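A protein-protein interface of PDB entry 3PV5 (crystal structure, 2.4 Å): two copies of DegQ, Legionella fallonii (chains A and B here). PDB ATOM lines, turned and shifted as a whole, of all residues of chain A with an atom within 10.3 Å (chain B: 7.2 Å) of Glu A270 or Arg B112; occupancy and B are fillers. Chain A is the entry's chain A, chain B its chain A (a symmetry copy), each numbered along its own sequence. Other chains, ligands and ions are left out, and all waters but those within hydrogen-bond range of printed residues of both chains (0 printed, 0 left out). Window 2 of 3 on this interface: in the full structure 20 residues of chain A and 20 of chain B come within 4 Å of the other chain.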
ATOM      1  N   GLN A 265      -1.689 -30.528  32.387  1.00  0.00           N
ATOM      2  CA  GLN A 265      -1.230 -30.059  31.060  1.00  0.00           C
ATOM      3  C   GLN A 265      -0.122 -29.016  31.138  1.00  0.00           C
ATOM      4  O   GLN A 265       0.009 -28.324  32.124  1.00  0.00           O
ATOM      5  CB  GLN A 265      -2.394 -29.618  30.099  1.00  0.00           C
ATOM      6  CG  GLN A 265      -2.794 -28.122  30.102  1.00  0.00           C
ATOM      7  CD  GLN A 265      -4.018 -27.799  29.270  1.00  0.00           C
ATOM      8  OE1 GLN A 265      -5.128 -28.072  29.720  1.00  0.00           O
ATOM      9  NE2 GLN A 265      -3.823 -27.223  27.998  1.00  0.00           N
ATOM     10  N   HIS A 266       0.707 -28.932  30.118  1.00  0.00           N
ATOM     11  CA  HIS A 266       1.750 -27.922  30.136  1.00  0.00           C
ATOM     12  C   HIS A 266       1.154 -26.531  30.244  1.00  0.00           C
ATOM     13  O   HIS A 266       0.324 -26.165  29.387  1.00  0.00           O
ATOM     14  CB  HIS A 266       2.636 -27.972  28.888  1.00  0.00           C
ATOM     15  CG  HIS A 266       3.793 -27.039  28.980  1.00  0.00           C
ATOM     16  ND1 HIS A 266       4.070 -26.084  28.019  1.00  0.00           N
ATOM     17  CD2 HIS A 266       4.702 -26.853  29.974  1.00  0.00           C
ATOM     18  CE1 HIS A 266       5.104 -25.355  28.422  1.00  0.00           C
ATOM     19  NE2 HIS A 266       5.508 -25.804  29.602  1.00  0.00           N
ATOM     20  N   LEU A 267       1.562 -25.750  31.267  1.00  0.00           N
ATOM     21  CA  LEU A 267       1.179 -24.348  31.365  1.00  0.00           C
ATOM     22  C   LEU A 267       2.062 -23.453  30.473  1.00  0.00           C
ATOM     23  O   LEU A 267       3.141 -23.027  30.877  1.00  0.00           O
ATOM     24  CB  LEU A 267       1.244 -23.858  32.813  1.00  0.00           C
ATOM     25  CG  LEU A 267       0.745 -22.418  33.072  1.00  0.00           C
ATOM     26  CD1 LEU A 267      -0.812 -22.436  33.039  1.00  0.00           C
ATOM     27  CD2 LEU A 267       1.263 -21.796  34.391  1.00  0.00           C
ATOM     28  N   THR A 268       1.585 -23.125  29.281  1.00  0.00           N
ATOM     29  CA  THR A 268       2.348 -22.241  28.376  1.00  0.00           C
ATOM     30  C   THR A 268       2.252 -20.790  28.860  1.00  0.00           C
ATOM     31  O   THR A 268       1.380 -20.437  29.647  1.00  0.00           O
ATOM     32  CB  THR A 268       1.767 -22.271  26.933  1.00  0.00           C
ATOM     33  OG1 THR A 268       0.395 -21.870  27.011  1.00  0.00           O
ATOM     34  CG2 THR A 268       1.890 -23.668  26.254  1.00  0.00           C
ATOM     35  N   PRO A 269       3.160 -19.937  28.400  1.00  0.00           N
ATOM     36  CA  PRO A 269       3.061 -18.547  28.735  1.00  0.00           C
ATOM     37  C   PRO A 269       1.707 -18.047  28.316  1.00  0.00           C
ATOM     38  O   PRO A 269       1.053 -17.385  29.070  1.00  0.00           O
ATOM     39  CB  PRO A 269       4.184 -17.907  27.890  1.00  0.00           C
ATOM     40  CG  PRO A 269       5.230 -19.000  27.867  1.00  0.00           C
ATOM     41  CD  PRO A 269       4.399 -20.235  27.663  1.00  0.00           C
ATOM     42  N   GLU A 270       1.284 -18.398  27.108  1.00  0.00           N
ATOM     43  CA  GLU A 270      -0.042 -18.019  26.610  1.00  0.00           C
ATOM     44  C   GLU A 270      -1.149 -18.310  27.609  1.00  0.00           C
ATOM     45  O   GLU A 270      -1.924 -17.467  27.913  1.00  0.00           O
ATOM     46  CB  GLU A 270      -0.373 -18.727  25.293  1.00  0.00           C
ATOM     47  CG  GLU A 270      -1.630 -18.094  24.669  1.00  0.00           C
ATOM     48  CD  GLU A 270      -2.136 -18.763  23.383  1.00  0.00           C
ATOM     49  OE1 GLU A 270      -2.020 -20.034  23.175  1.00  0.00           O
ATOM     50  OE2 GLU A 270      -2.703 -17.955  22.604  1.00  0.00           O
ATOM     51  N   LEU A 271      -1.191 -19.532  28.096  1.00  0.00           N
ATOM     52  CA  LEU A 271      -2.207 -19.968  29.020  1.00  0.00           C
ATOM     53  C   LEU A 271      -2.065 -19.289  30.394  1.00  0.00           C
ATOM     54  O   LEU A 271      -3.043 -18.839  30.969  1.00  0.00           O
ATOM     55  CB  LEU A 271      -2.095 -21.482  29.184  1.00  0.00           C
ATOM     56  CG  LEU A 271      -3.072 -22.494  28.575  1.00  0.00           C
ATOM     57  CD1 LEU A 271      -4.196 -21.907  27.751  1.00  0.00           C
ATOM     58  CD2 LEU A 271      -2.313 -23.602  27.839  1.00  0.00           C
ATOM     59  N   ALA A 272      -0.844 -19.214  30.923  1.00  0.00           N
ATOM     60  CA  ALA A 272      -0.609 -18.465  32.155  1.00  0.00           C
ATOM     61  C   ALA A 272      -1.270 -17.062  32.098  1.00  0.00           C
ATOM     62  O   ALA A 272      -2.070 -16.700  32.976  1.00  0.00           O
ATOM     63  CB  ALA A 272       0.909 -18.364  32.421  1.00  0.00           C
ATOM     64  N   GLN A 273      -0.976 -16.308  31.040  1.00  0.00           N
ATOM     65  CA  GLN A 273      -1.489 -14.947  30.916  1.00  0.00           C
ATOM     66  C   GLN A 273      -3.001 -14.964  30.796  1.00  0.00           C
ATOM     67  O   GLN A 273      -3.673 -14.240  31.534  1.00  0.00           O
ATOM     68  CB  GLN A 273      -0.877 -14.185  29.749  1.00  0.00           C
ATOM     69  CG  GLN A 273       0.504 -13.601  30.066  1.00  0.00           C
ATOM     70  CD  GLN A 273       1.237 -13.055  28.815  1.00  0.00           C
ATOM     71  OE1 GLN A 273       1.300 -13.717  27.753  1.00  0.00           O
ATOM     72  NE2 GLN A 273       1.839 -11.866  28.961  1.00  0.00           N
ATOM     73  N   ALA A 274      -3.547 -15.851  29.950  1.00  0.00           N
ATOM     74  CA  ALA A 274      -5.004 -15.908  29.796  1.00  0.00           C
ATOM     75  C   ALA A 274      -5.687 -16.307  31.108  1.00  0.00           C
ATOM     76  O   ALA A 274      -6.865 -16.053  31.304  1.00  0.00           O
ATOM     77  CB  ALA A 274      -5.431 -16.851  28.614  1.00  0.00           C
ATOM     78  N   MET A 275      -4.956 -16.932  32.007  1.00  0.00           N
ATOM     79  CA  MET A 275      -5.520 -17.293  33.295  1.00  0.00           C
ATOM     80  C   MET A 275      -5.206 -16.339  34.461  1.00  0.00           C
ATOM     81  O   MET A 275      -5.658 -16.546  35.573  1.00  0.00           O
ATOM     82  CB  MET A 275      -5.102 -18.678  33.610  1.00  0.00           C
ATOM     83  CG  MET A 275      -5.776 -19.648  32.655  1.00  0.00           C
ATOM     84  SD  MET A 275      -5.288 -21.275  33.064  1.00  0.00           S
ATOM     85  CE  MET A 275      -6.315 -21.302  34.662  1.00  0.00           C
ATOM     86  N   GLY A 276      -4.449 -15.284  34.156  1.00  0.00           N
ATOM     87  CA  GLY A 276      -4.293 -14.126  35.036  1.00  0.00           C
ATOM     88  C   GLY A 276      -3.038 -14.153  35.883  1.00  0.00           C
ATOM     89  O   GLY A 276      -3.105 -13.748  37.020  1.00  0.00           O
ATOM     90  N   TYR A 277      -1.943 -14.660  35.309  1.00  0.00           N
ATOM     91  CA  TYR A 277      -0.636 -14.832  35.918  1.00  0.00           C
ATOM     92  C   TYR A 277       0.372 -14.303  34.868  1.00  0.00           C
ATOM     93  O   TYR A 277       0.067 -14.258  33.695  1.00  0.00           O
ATOM     94  CB  TYR A 277      -0.317 -16.299  36.152  1.00  0.00           C
ATOM     95  CG  TYR A 277      -1.275 -17.009  37.032  1.00  0.00           C
ATOM     96  CD1 TYR A 277      -2.386 -17.630  36.512  1.00  0.00           C
ATOM     97  CD2 TYR A 277      -1.081 -17.081  38.394  1.00  0.00           C
ATOM     98  CE1 TYR A 277      -3.286 -18.301  37.328  1.00  0.00           C
ATOM     99  CE2 TYR A 277      -1.968 -17.732  39.205  1.00  0.00           C
ATOM    100  CZ  TYR A 277      -3.083 -18.337  38.667  1.00  0.00           C
ATOM    101  OH  TYR A 277      -4.018 -18.992  39.464  1.00  0.00           O
ATOM    102  N   PRO A 278       1.565 -13.885  35.296  1.00  0.00           N
ATOM    103  CA  PRO A 278       2.635 -13.449  34.400  1.00  0.00           C
ATOM    104  C   PRO A 278       3.140 -14.513  33.393  1.00  0.00           C
ATOM    105  O   PRO A 278       3.088 -15.736  33.661  1.00  0.00           O
ATOM    106  CB  PRO A 278       3.789 -13.126  35.380  1.00  0.00           C
ATOM    107  CG  PRO A 278       3.147 -12.902  36.696  1.00  0.00           C
ATOM    108  CD  PRO A 278       1.982 -13.862  36.705  1.00  0.00           C
ATOM    109  N   GLU A 279       3.707 -14.025  32.295  1.00  0.00           N
ATOM    110  CA  GLU A 279       4.169 -14.873  31.207  1.00  0.00           C
ATOM    111  C   GLU A 279       5.154 -15.932  31.663  1.00  0.00           C
ATOM    112  O   GLU A 279       5.173 -17.023  31.153  1.00  0.00           O
ATOM    113  CB  GLU A 279       4.771 -14.035  30.048  1.00  0.00           C
ATOM    114  CG  GLU A 279       5.991 -13.126  30.408  1.00  0.00           C
ATOM    115  CD  GLU A 279       6.623 -12.410  29.177  1.00  0.00           C
ATOM    116  OE1 GLU A 279       5.917 -12.307  28.135  1.00  0.00           O
ATOM    117  OE2 GLU A 279       7.823 -11.950  29.253  1.00  0.00           O
ATOM    118  N   ASP A 280       5.961 -15.617  32.641  1.00  0.00           N
ATOM    119  CA  ASP A 280       7.007 -16.518  33.082  1.00  0.00           C
ATOM    120  C   ASP A 280       6.545 -17.401  34.244  1.00  0.00           C
ATOM    121  O   ASP A 280       7.348 -18.139  34.788  1.00  0.00           O
ATOM    122  CB  ASP A 280       8.281 -15.725  33.482  1.00  0.00           C
ATOM    123  CG  ASP A 280       8.014 -14.675  34.556  1.00  0.00           C
ATOM    124  OD1 ASP A 280       6.830 -14.318  34.793  1.00  0.00           O
ATOM    125  OD2 ASP A 280       8.993 -14.181  35.161  1.00  0.00           O
ATOM    126  N   PHE A 281       5.271 -17.333  34.624  1.00  0.00           N
ATOM    127  CA  PHE A 281       4.807 -18.136  35.760  1.00  0.00           C
ATOM    128  C   PHE A 281       4.865 -19.626  35.426  1.00  0.00           C
ATOM    129  O   PHE A 281       4.554 -20.025  34.312  1.00  0.00           O
ATOM    130  CB  PHE A 281       3.396 -17.743  36.165  1.00  0.00           C
ATOM    131  CG  PHE A 281       2.975 -18.303  37.468  1.00  0.00           C
ATOM    132  CD1 PHE A 281       2.198 -19.454  37.531  1.00  0.00           C
ATOM    133  CD2 PHE A 281       3.352 -17.690  38.656  1.00  0.00           C
ATOM    134  CE1 PHE A 281       1.771 -19.980  38.767  1.00  0.00           C
ATOM    135  CE2 PHE A 281       2.942 -18.210  39.904  1.00  0.00           C
ATOM    136  CZ  PHE A 281       2.145 -19.357  39.955  1.00  0.00           C
ATOM    137  N   LEU A 285      -0.864 -27.249  34.972  1.00  0.00           N
ATOM    138  CA  LEU A 285      -2.263 -26.903  34.841  1.00  0.00           C
ATOM    139  C   LEU A 285      -3.065 -28.174  34.988  1.00  0.00           C
ATOM    140  O   LEU A 285      -2.818 -29.170  34.305  1.00  0.00           O
ATOM    141  CB  LEU A 285      -2.506 -26.229  33.509  1.00  0.00           C
ATOM    142  CG  LEU A 285      -3.935 -25.735  33.180  1.00  0.00           C
ATOM    143  CD1 LEU A 285      -4.585 -24.926  34.313  1.00  0.00           C
ATOM    144  CD2 LEU A 285      -3.936 -24.951  31.828  1.00  0.00           C
ATOM    145  N   ILE A 305      -3.467 -24.455  39.372  1.00  0.00           N
ATOM    146  CA  ILE A 305      -2.109 -24.627  38.875  1.00  0.00           C
ATOM    147  C   ILE A 305      -1.232 -25.180  39.956  1.00  0.00           C
ATOM    148  O   ILE A 305      -0.938 -24.468  40.932  1.00  0.00           O
ATOM    149  CB  ILE A 305      -1.518 -23.362  38.391  1.00  0.00           C
ATOM    150  CG1 ILE A 305      -2.253 -22.914  37.112  1.00  0.00           C
ATOM    151  CG2 ILE A 305      -0.042 -23.597  38.108  1.00  0.00           C
ATOM    152  CD1 ILE A 305      -2.052 -21.449  36.815  1.00  0.00           C
ATOM    153  N   THR B 105      -0.384 -22.203   9.240  1.00  0.00           N
ATOM    154  CA  THR B 105      -0.405 -21.850  10.671  1.00  0.00           C
ATOM    155  C   THR B 105       0.975 -21.962  11.350  1.00  0.00           C
ATOM    156  O   THR B 105       1.544 -23.036  11.373  1.00  0.00           O
ATOM    157  CB  THR B 105      -1.251 -22.884  11.440  1.00  0.00           C
ATOM    158  OG1 THR B 105      -2.525 -22.934  10.874  1.00  0.00           O
ATOM    159  CG2 THR B 105      -1.376 -22.536  12.871  1.00  0.00           C
ATOM    160  N   VAL B 106       1.428 -20.855  11.930  1.00  0.00           N
ATOM    161  CA  VAL B 106       2.631 -20.708  12.741  1.00  0.00           C
ATOM    162  C   VAL B 106       2.293 -20.899  14.237  1.00  0.00           C
ATOM    163  O   VAL B 106       1.306 -20.298  14.775  1.00  0.00           O
ATOM    164  CB  VAL B 106       3.229 -19.323  12.475  1.00  0.00           C
ATOM    165  CG1 VAL B 106       4.289 -18.928  13.457  1.00  0.00           C
ATOM    166  CG2 VAL B 106       3.818 -19.259  11.041  1.00  0.00           C
ATOM    167  N   THR B 107       3.050 -21.798  14.880  1.00  0.00           N
ATOM    168  CA  THR B 107       3.003 -22.028  16.322  1.00  0.00           C
ATOM    169  C   THR B 107       4.280 -21.444  16.882  1.00  0.00           C
ATOM    170  O   THR B 107       5.333 -21.757  16.386  1.00  0.00           O
ATOM    171  CB  THR B 107       2.898 -23.526  16.652  1.00  0.00           C
ATOM    172  OG1 THR B 107       1.636 -24.058  16.159  1.00  0.00           O
ATOM    173  CG2 THR B 107       2.971 -23.757  18.183  1.00  0.00           C
ATOM    174  N   LEU B 108       4.178 -20.532  17.840  1.00  0.00           N
ATOM    175  CA  LEU B 108       5.303 -19.961  18.562  1.00  0.00           C
ATOM    176  C   LEU B 108       5.627 -20.779  19.793  1.00  0.00           C
ATOM    177  O   LEU B 108       4.784 -21.524  20.239  1.00  0.00           O
ATOM    178  CB  LEU B 108       4.981 -18.550  19.040  1.00  0.00           C
ATOM    179  CG  LEU B 108       4.573 -17.515  17.979  1.00  0.00           C
ATOM    180  CD1 LEU B 108       4.475 -16.151  18.631  1.00  0.00           C
ATOM    181  CD2 LEU B 108       5.528 -17.479  16.710  1.00  0.00           C
ATOM    182  N   GLN B 109       6.857 -20.646  20.305  1.00  0.00           N
ATOM    183  CA  GLN B 109       7.316 -21.292  21.540  1.00  0.00           C
ATOM    184  C   GLN B 109       6.377 -20.963  22.699  1.00  0.00           C
ATOM    185  O   GLN B 109       6.079 -21.844  23.494  1.00  0.00           O
ATOM    186  CB  GLN B 109       8.740 -20.798  21.909  1.00  0.00           C
ATOM    187  CG  GLN B 109       9.392 -21.472  23.132  1.00  0.00           C
ATOM    188  CD  GLN B 109      10.601 -20.694  23.670  1.00  0.00           C
ATOM    189  OE1 GLN B 109      11.640 -21.270  23.941  1.00  0.00           O
ATOM    190  NE2 GLN B 109      10.465 -19.379  23.808  1.00  0.00           N
ATOM    191  N   ASP B 110       5.883 -19.699  22.734  1.00  0.00           N
ATOM    192  CA  ASP B 110       4.938 -19.231  23.744  1.00  0.00           C
ATOM    193  C   ASP B 110       3.556 -19.850  23.706  1.00  0.00           C
ATOM    194  O   ASP B 110       2.807 -19.695  24.627  1.00  0.00           O
ATOM    195  CB  ASP B 110       4.835 -17.686  23.744  1.00  0.00           C
ATOM    196  CG  ASP B 110       4.020 -17.174  22.622  1.00  0.00           C
ATOM    197  OD1 ASP B 110       3.238 -17.972  22.047  1.00  0.00           O
ATOM    198  OD2 ASP B 110       4.158 -15.970  22.307  1.00  0.00           O
ATOM    199  N   GLY B 111       3.212 -20.565  22.671  1.00  0.00           N
ATOM    200  CA  GLY B 111       1.932 -21.295  22.638  1.00  0.00           C
ATOM    201  C   GLY B 111       0.951 -20.827  21.552  1.00  0.00           C
ATOM    202  O   GLY B 111       0.095 -21.573  21.126  1.00  0.00           O
ATOM    203  N   ARG B 112       1.048 -19.583  21.114  1.00  0.00           N
ATOM    204  CA  ARG B 112       0.055 -19.073  20.165  1.00  0.00           C
ATOM    205  C   ARG B 112       0.104 -19.887  18.849  1.00  0.00           C
ATOM    206  O   ARG B 112       1.220 -20.207  18.329  1.00  0.00           O
ATOM    207  CB  ARG B 112       0.328 -17.585  19.917  1.00  0.00           C
ATOM    208  CG  ARG B 112      -0.011 -16.600  21.128  1.00  0.00           C
ATOM    209  CD  ARG B 112       0.378 -15.159  20.825  1.00  0.00           C
ATOM    210  NE  ARG B 112       1.789 -14.893  21.102  1.00  0.00           N
ATOM    211  CZ  ARG B 112       2.456 -13.781  20.793  1.00  0.00           C
ATOM    212  NH1 ARG B 112       1.897 -12.767  20.156  1.00  0.00           N
ATOM    213  NH2 ARG B 112       3.730 -13.679  21.109  1.00  0.00           N
ATOM    214  N   ARG B 113      -1.072 -20.304  18.363  1.00  0.00           N
ATOM    215  CA  ARG B 113      -1.178 -20.833  17.022  1.00  0.00           C
ATOM    216  C   ARG B 113      -1.829 -19.748  16.113  1.00  0.00           C
ATOM    217  O   ARG B 113      -2.996 -19.413  16.284  1.00  0.00           O
ATOM    218  CB  ARG B 113      -1.879 -22.167  17.007  1.00  0.00           C
ATOM    219  CG  ARG B 113      -1.467 -23.043  18.196  1.00  0.00           C
ATOM    220  CD  ARG B 113      -1.191 -24.531  17.905  1.00  0.00           C
ATOM    221  NE  ARG B 113      -2.121 -25.151  16.950  1.00  0.00           N
ATOM    222  CZ  ARG B 113      -1.809 -25.649  15.739  1.00  0.00           C
ATOM    223  NH1 ARG B 113      -0.568 -25.630  15.266  1.00  0.00           N
ATOM    224  NH2 ARG B 113      -2.762 -26.174  14.979  1.00  0.00           N
ATOM    225  N   LEU B 114      -1.037 -19.207  15.161  1.00  0.00           N
ATOM    226  CA  LEU B 114      -1.359 -17.996  14.384  1.00  0.00           C
ATOM    227  C   LEU B 114      -1.528 -18.286  12.900  1.00  0.00           C
ATOM    228  O   LEU B 114      -0.680 -18.953  12.290  1.00  0.00           O
ATOM    229  CB  LEU B 114      -0.180 -17.021  14.497  1.00  0.00           C
ATOM    230  CG  LEU B 114      -0.009 -16.435  15.888  1.00  0.00           C
ATOM    231  CD1 LEU B 114       1.353 -15.887  16.084  1.00  0.00           C
ATOM    232  CD2 LEU B 114      -1.182 -15.357  16.105  1.00  0.00           C
ATOM    233  N   ILE B 132       2.797 -12.864   9.921  1.00  0.00           N
ATOM    234  CA  ILE B 132       1.784 -13.120  10.980  1.00  0.00           C
ATOM    235  C   ILE B 132       1.534 -11.789  11.645  1.00  0.00           C
ATOM    236  O   ILE B 132       2.445 -10.970  11.722  1.00  0.00           O
ATOM    237  CB  ILE B 132       2.246 -14.111  12.077  1.00  0.00           C
ATOM    238  CG1 ILE B 132       3.571 -13.698  12.706  1.00  0.00           C
ATOM    239  CG2 ILE B 132       2.356 -15.441  11.526  1.00  0.00           C
ATOM    240  CD1 ILE B 132       4.019 -14.661  13.910  1.00  0.00           C
ATOM    241  N   ASP B 133       0.296 -11.521  12.087  1.00  0.00           N
ATOM    242  CA  ASP B 133       0.029 -10.215  12.745  1.00  0.00           C
ATOM    243  C   ASP B 133      -0.061 -10.519  14.255  1.00  0.00           C
ATOM    244  O   ASP B 133      -0.986 -11.196  14.709  1.00  0.00           O
ATOM    245  CB  ASP B 133      -1.247  -9.553  12.187  1.00  0.00           C
ATOM    246  CG  ASP B 133      -1.197  -9.318  10.647  1.00  0.00           C
ATOM    247  OD1 ASP B 133      -2.117  -9.786   9.927  1.00  0.00           O
ATOM    248  OD2 ASP B 133      -0.275  -8.640  10.126  1.00  0.00           O
ATOM    249  N   ALA B 134       0.923 -10.077  15.015  1.00  0.00           N
ATOM    250  CA  ALA B 134       1.023 -10.436  16.438  1.00  0.00           C
ATOM    251  C   ALA B 134       2.111  -9.625  17.075  1.00  0.00           C
ATOM    252  O   ALA B 134       3.052  -9.188  16.402  1.00  0.00           O
ATOM    253  CB  ALA B 134       1.316 -11.861  16.598  1.00  0.00           C
ATOM    254  N   LYS B 135       2.001  -9.414  18.384  1.00  0.00           N
ATOM    255  CA  LYS B 135       2.992  -8.570  19.061  1.00  0.00           C
ATOM    256  C   LYS B 135       3.770  -9.424  20.018  1.00  0.00           C
ATOM    257  O   LYS B 135       3.580 -10.656  20.102  1.00  0.00           O
ATOM    258  CB  LYS B 135       2.317  -7.404  19.777  1.00  0.00           C
ATOM    259  CG  LYS B 135       1.407  -6.608  18.854  1.00  0.00           C
ATOM    260  CD  LYS B 135       0.824  -5.370  19.506  1.00  0.00           C
ATOM    261  CE  LYS B 135       0.291  -4.434  18.424  1.00  0.00           C
ATOM    262  NZ  LYS B 135      -0.927  -4.998  17.803  1.00  0.00           N
ATOM    263  N   ASN B 136       4.642  -8.776  20.762  1.00  0.00           N
ATOM    264  CA  ASN B 136       5.510  -9.533  21.638  1.00  0.00           C
ATOM    265  C   ASN B 136       6.214 -10.720  20.933  1.00  0.00           C
ATOM    266  O   ASN B 136       6.058 -11.878  21.265  1.00  0.00           O
ATOM    267  CB  ASN B 136       4.741 -10.048  22.841  1.00  0.00           C
ATOM    268  CG  ASN B 136       5.657 -10.328  23.970  1.00  0.00           C
ATOM    269  OD1 ASN B 136       6.585  -9.509  24.254  1.00  0.00           O
ATOM    270  ND2 ASN B 136       5.475 -11.491  24.608  1.00  0.00           N
ATOM    271  N   LEU B 137       6.934 -10.383  19.892  1.00  0.00           N
ATOM    272  CA  LEU B 137       7.650 -11.368  19.132  1.00  0.00           C
ATOM    273  C   LEU B 137       9.136 -11.140  19.331  1.00  0.00           C
ATOM    274  O   LEU B 137       9.618 -10.009  19.545  1.00  0.00           O
ATOM    275  CB  LEU B 137       7.308 -11.176  17.687  1.00  0.00           C
ATOM    276  CG  LEU B 137       6.473 -12.151  16.886  1.00  0.00           C
ATOM    277  CD1 LEU B 137       5.466 -13.001  17.623  1.00  0.00           C
ATOM    278  CD2 LEU B 137       5.850 -11.306  15.736  1.00  0.00           C
ATOM    279  N   LYS B 138       9.856 -12.238  19.227  1.00  0.00           N
ATOM    280  CA  LYS B 138      11.299 -12.219  19.293  1.00  0.00           C
ATOM    281  C   LYS B 138      11.994 -12.695  17.984  1.00  0.00           C
ATOM    282  O   LYS B 138      11.509 -13.606  17.281  1.00  0.00           O
ATOM    283  CB  LYS B 138      11.735 -13.126  20.439  1.00  0.00           C
ATOM    284  CG  LYS B 138      10.990 -12.931  21.774  1.00  0.00           C
ATOM    285  CD  LYS B 138      11.655 -11.853  22.639  1.00  0.00           C
ATOM    286  CE  LYS B 138      11.207 -11.977  24.126  1.00  0.00           C
ATOM    287  NZ  LYS B 138       9.751 -11.643  24.350  1.00  0.00           N
ATOM    288  N   ASN B 168       5.529 -27.087  20.884  1.00  0.00           N
ATOM    289  CA  ASN B 168       6.101 -25.714  20.748  1.00  0.00           C
ATOM    290  C   ASN B 168       7.625 -25.714  21.014  1.00  0.00           C
ATOM    291  O   ASN B 168       8.205 -24.690  21.420  1.00  0.00           O
ATOM    292  CB  ASN B 168       5.447 -24.661  21.694  1.00  0.00           C
ATOM    293  CG  ASN B 168       3.885 -24.573  21.590  1.00  0.00           C
ATOM    294  OD1 ASN B 168       3.342 -23.614  21.033  1.00  0.00           O
ATOM    295  ND2 ASN B 168       3.185 -25.529  22.192  1.00  0.00           N
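N of Glu A270 is in hydrogen-bond range of O of Asp B110 (3.2 Å). The backbone carbonyl oxygen of Gly B111 lies close to the side-chain carboxylate of Glu A270, 3.3 Å away.
OG1 of Thr A268 is in hydrogen-bond range of N of Leu A271 (3.0 Å). OD2 of Asp B110 lies within salt-bridge range of NH2 of Arg B112, at 2.6 Å. N of Gly B111 lies close to OD1 of Asn B168, at 3.5 Å. O of Asn B136 is in hydrogen-bond range of NH2 of Arg B112 (2.9 Å). The backbone carbonyl oxygen of Lys B135 lies within hydrogen-bond range of the guanidinium group of Arg B112, at 2.7 Å.
O of Asp B110 touches CB of Thr A268, 3.6 Å away. Pro A269 touches Asp B110. Glu A270 touches Arg B112. Glu A279 touches Asn B136 (OE1 to ND2, 3.6 Å).
Of the printed residues of chain B, Thr A268 touches Asp B110 (3.6 Å). Printed residues of chain B within 4 Å of Pro A269: Asp B110. Glu A270 touches just these residues of chain B: Asp B110 (3.2 Å), Gly B111 (3.3 Å) and Arg B112 (3.4 Å). Of the printed residues of chain B, Glu A279 touches Asn B136 (3.6 Å). No residue of chain A comes within 4 Å of Leu B108. Of chain A, only Thr A268 (3.6 Å), Pro A269 (3.5 Å) and Glu A270 (3.2 Å) come within 4 Å of Asp B110. Gly B111 touches one residue of chain A. Arg B112 touches just one residue of chain A: Glu A270 (3.4 Å). No residue of chain A comes within 4 Å of Ala B134. Lys B135 touches none of the printed residues of chain A. The nearest printed residue of chain B that does not touch Glu A279 is Lys B138 (5.3 Å).
Printed residues of chain A that touch a printed residue of chain B: Thr A268, Pro A269, Glu A270 and Glu A279. Hydrophobic or aromatic side chains of chain A that line the printed part of chain B: Pro A269.
No position is printed for both chains. Of the 6 pairs that touch across the chains among the printed residues, none has its exchanged pair printed and touching as well.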
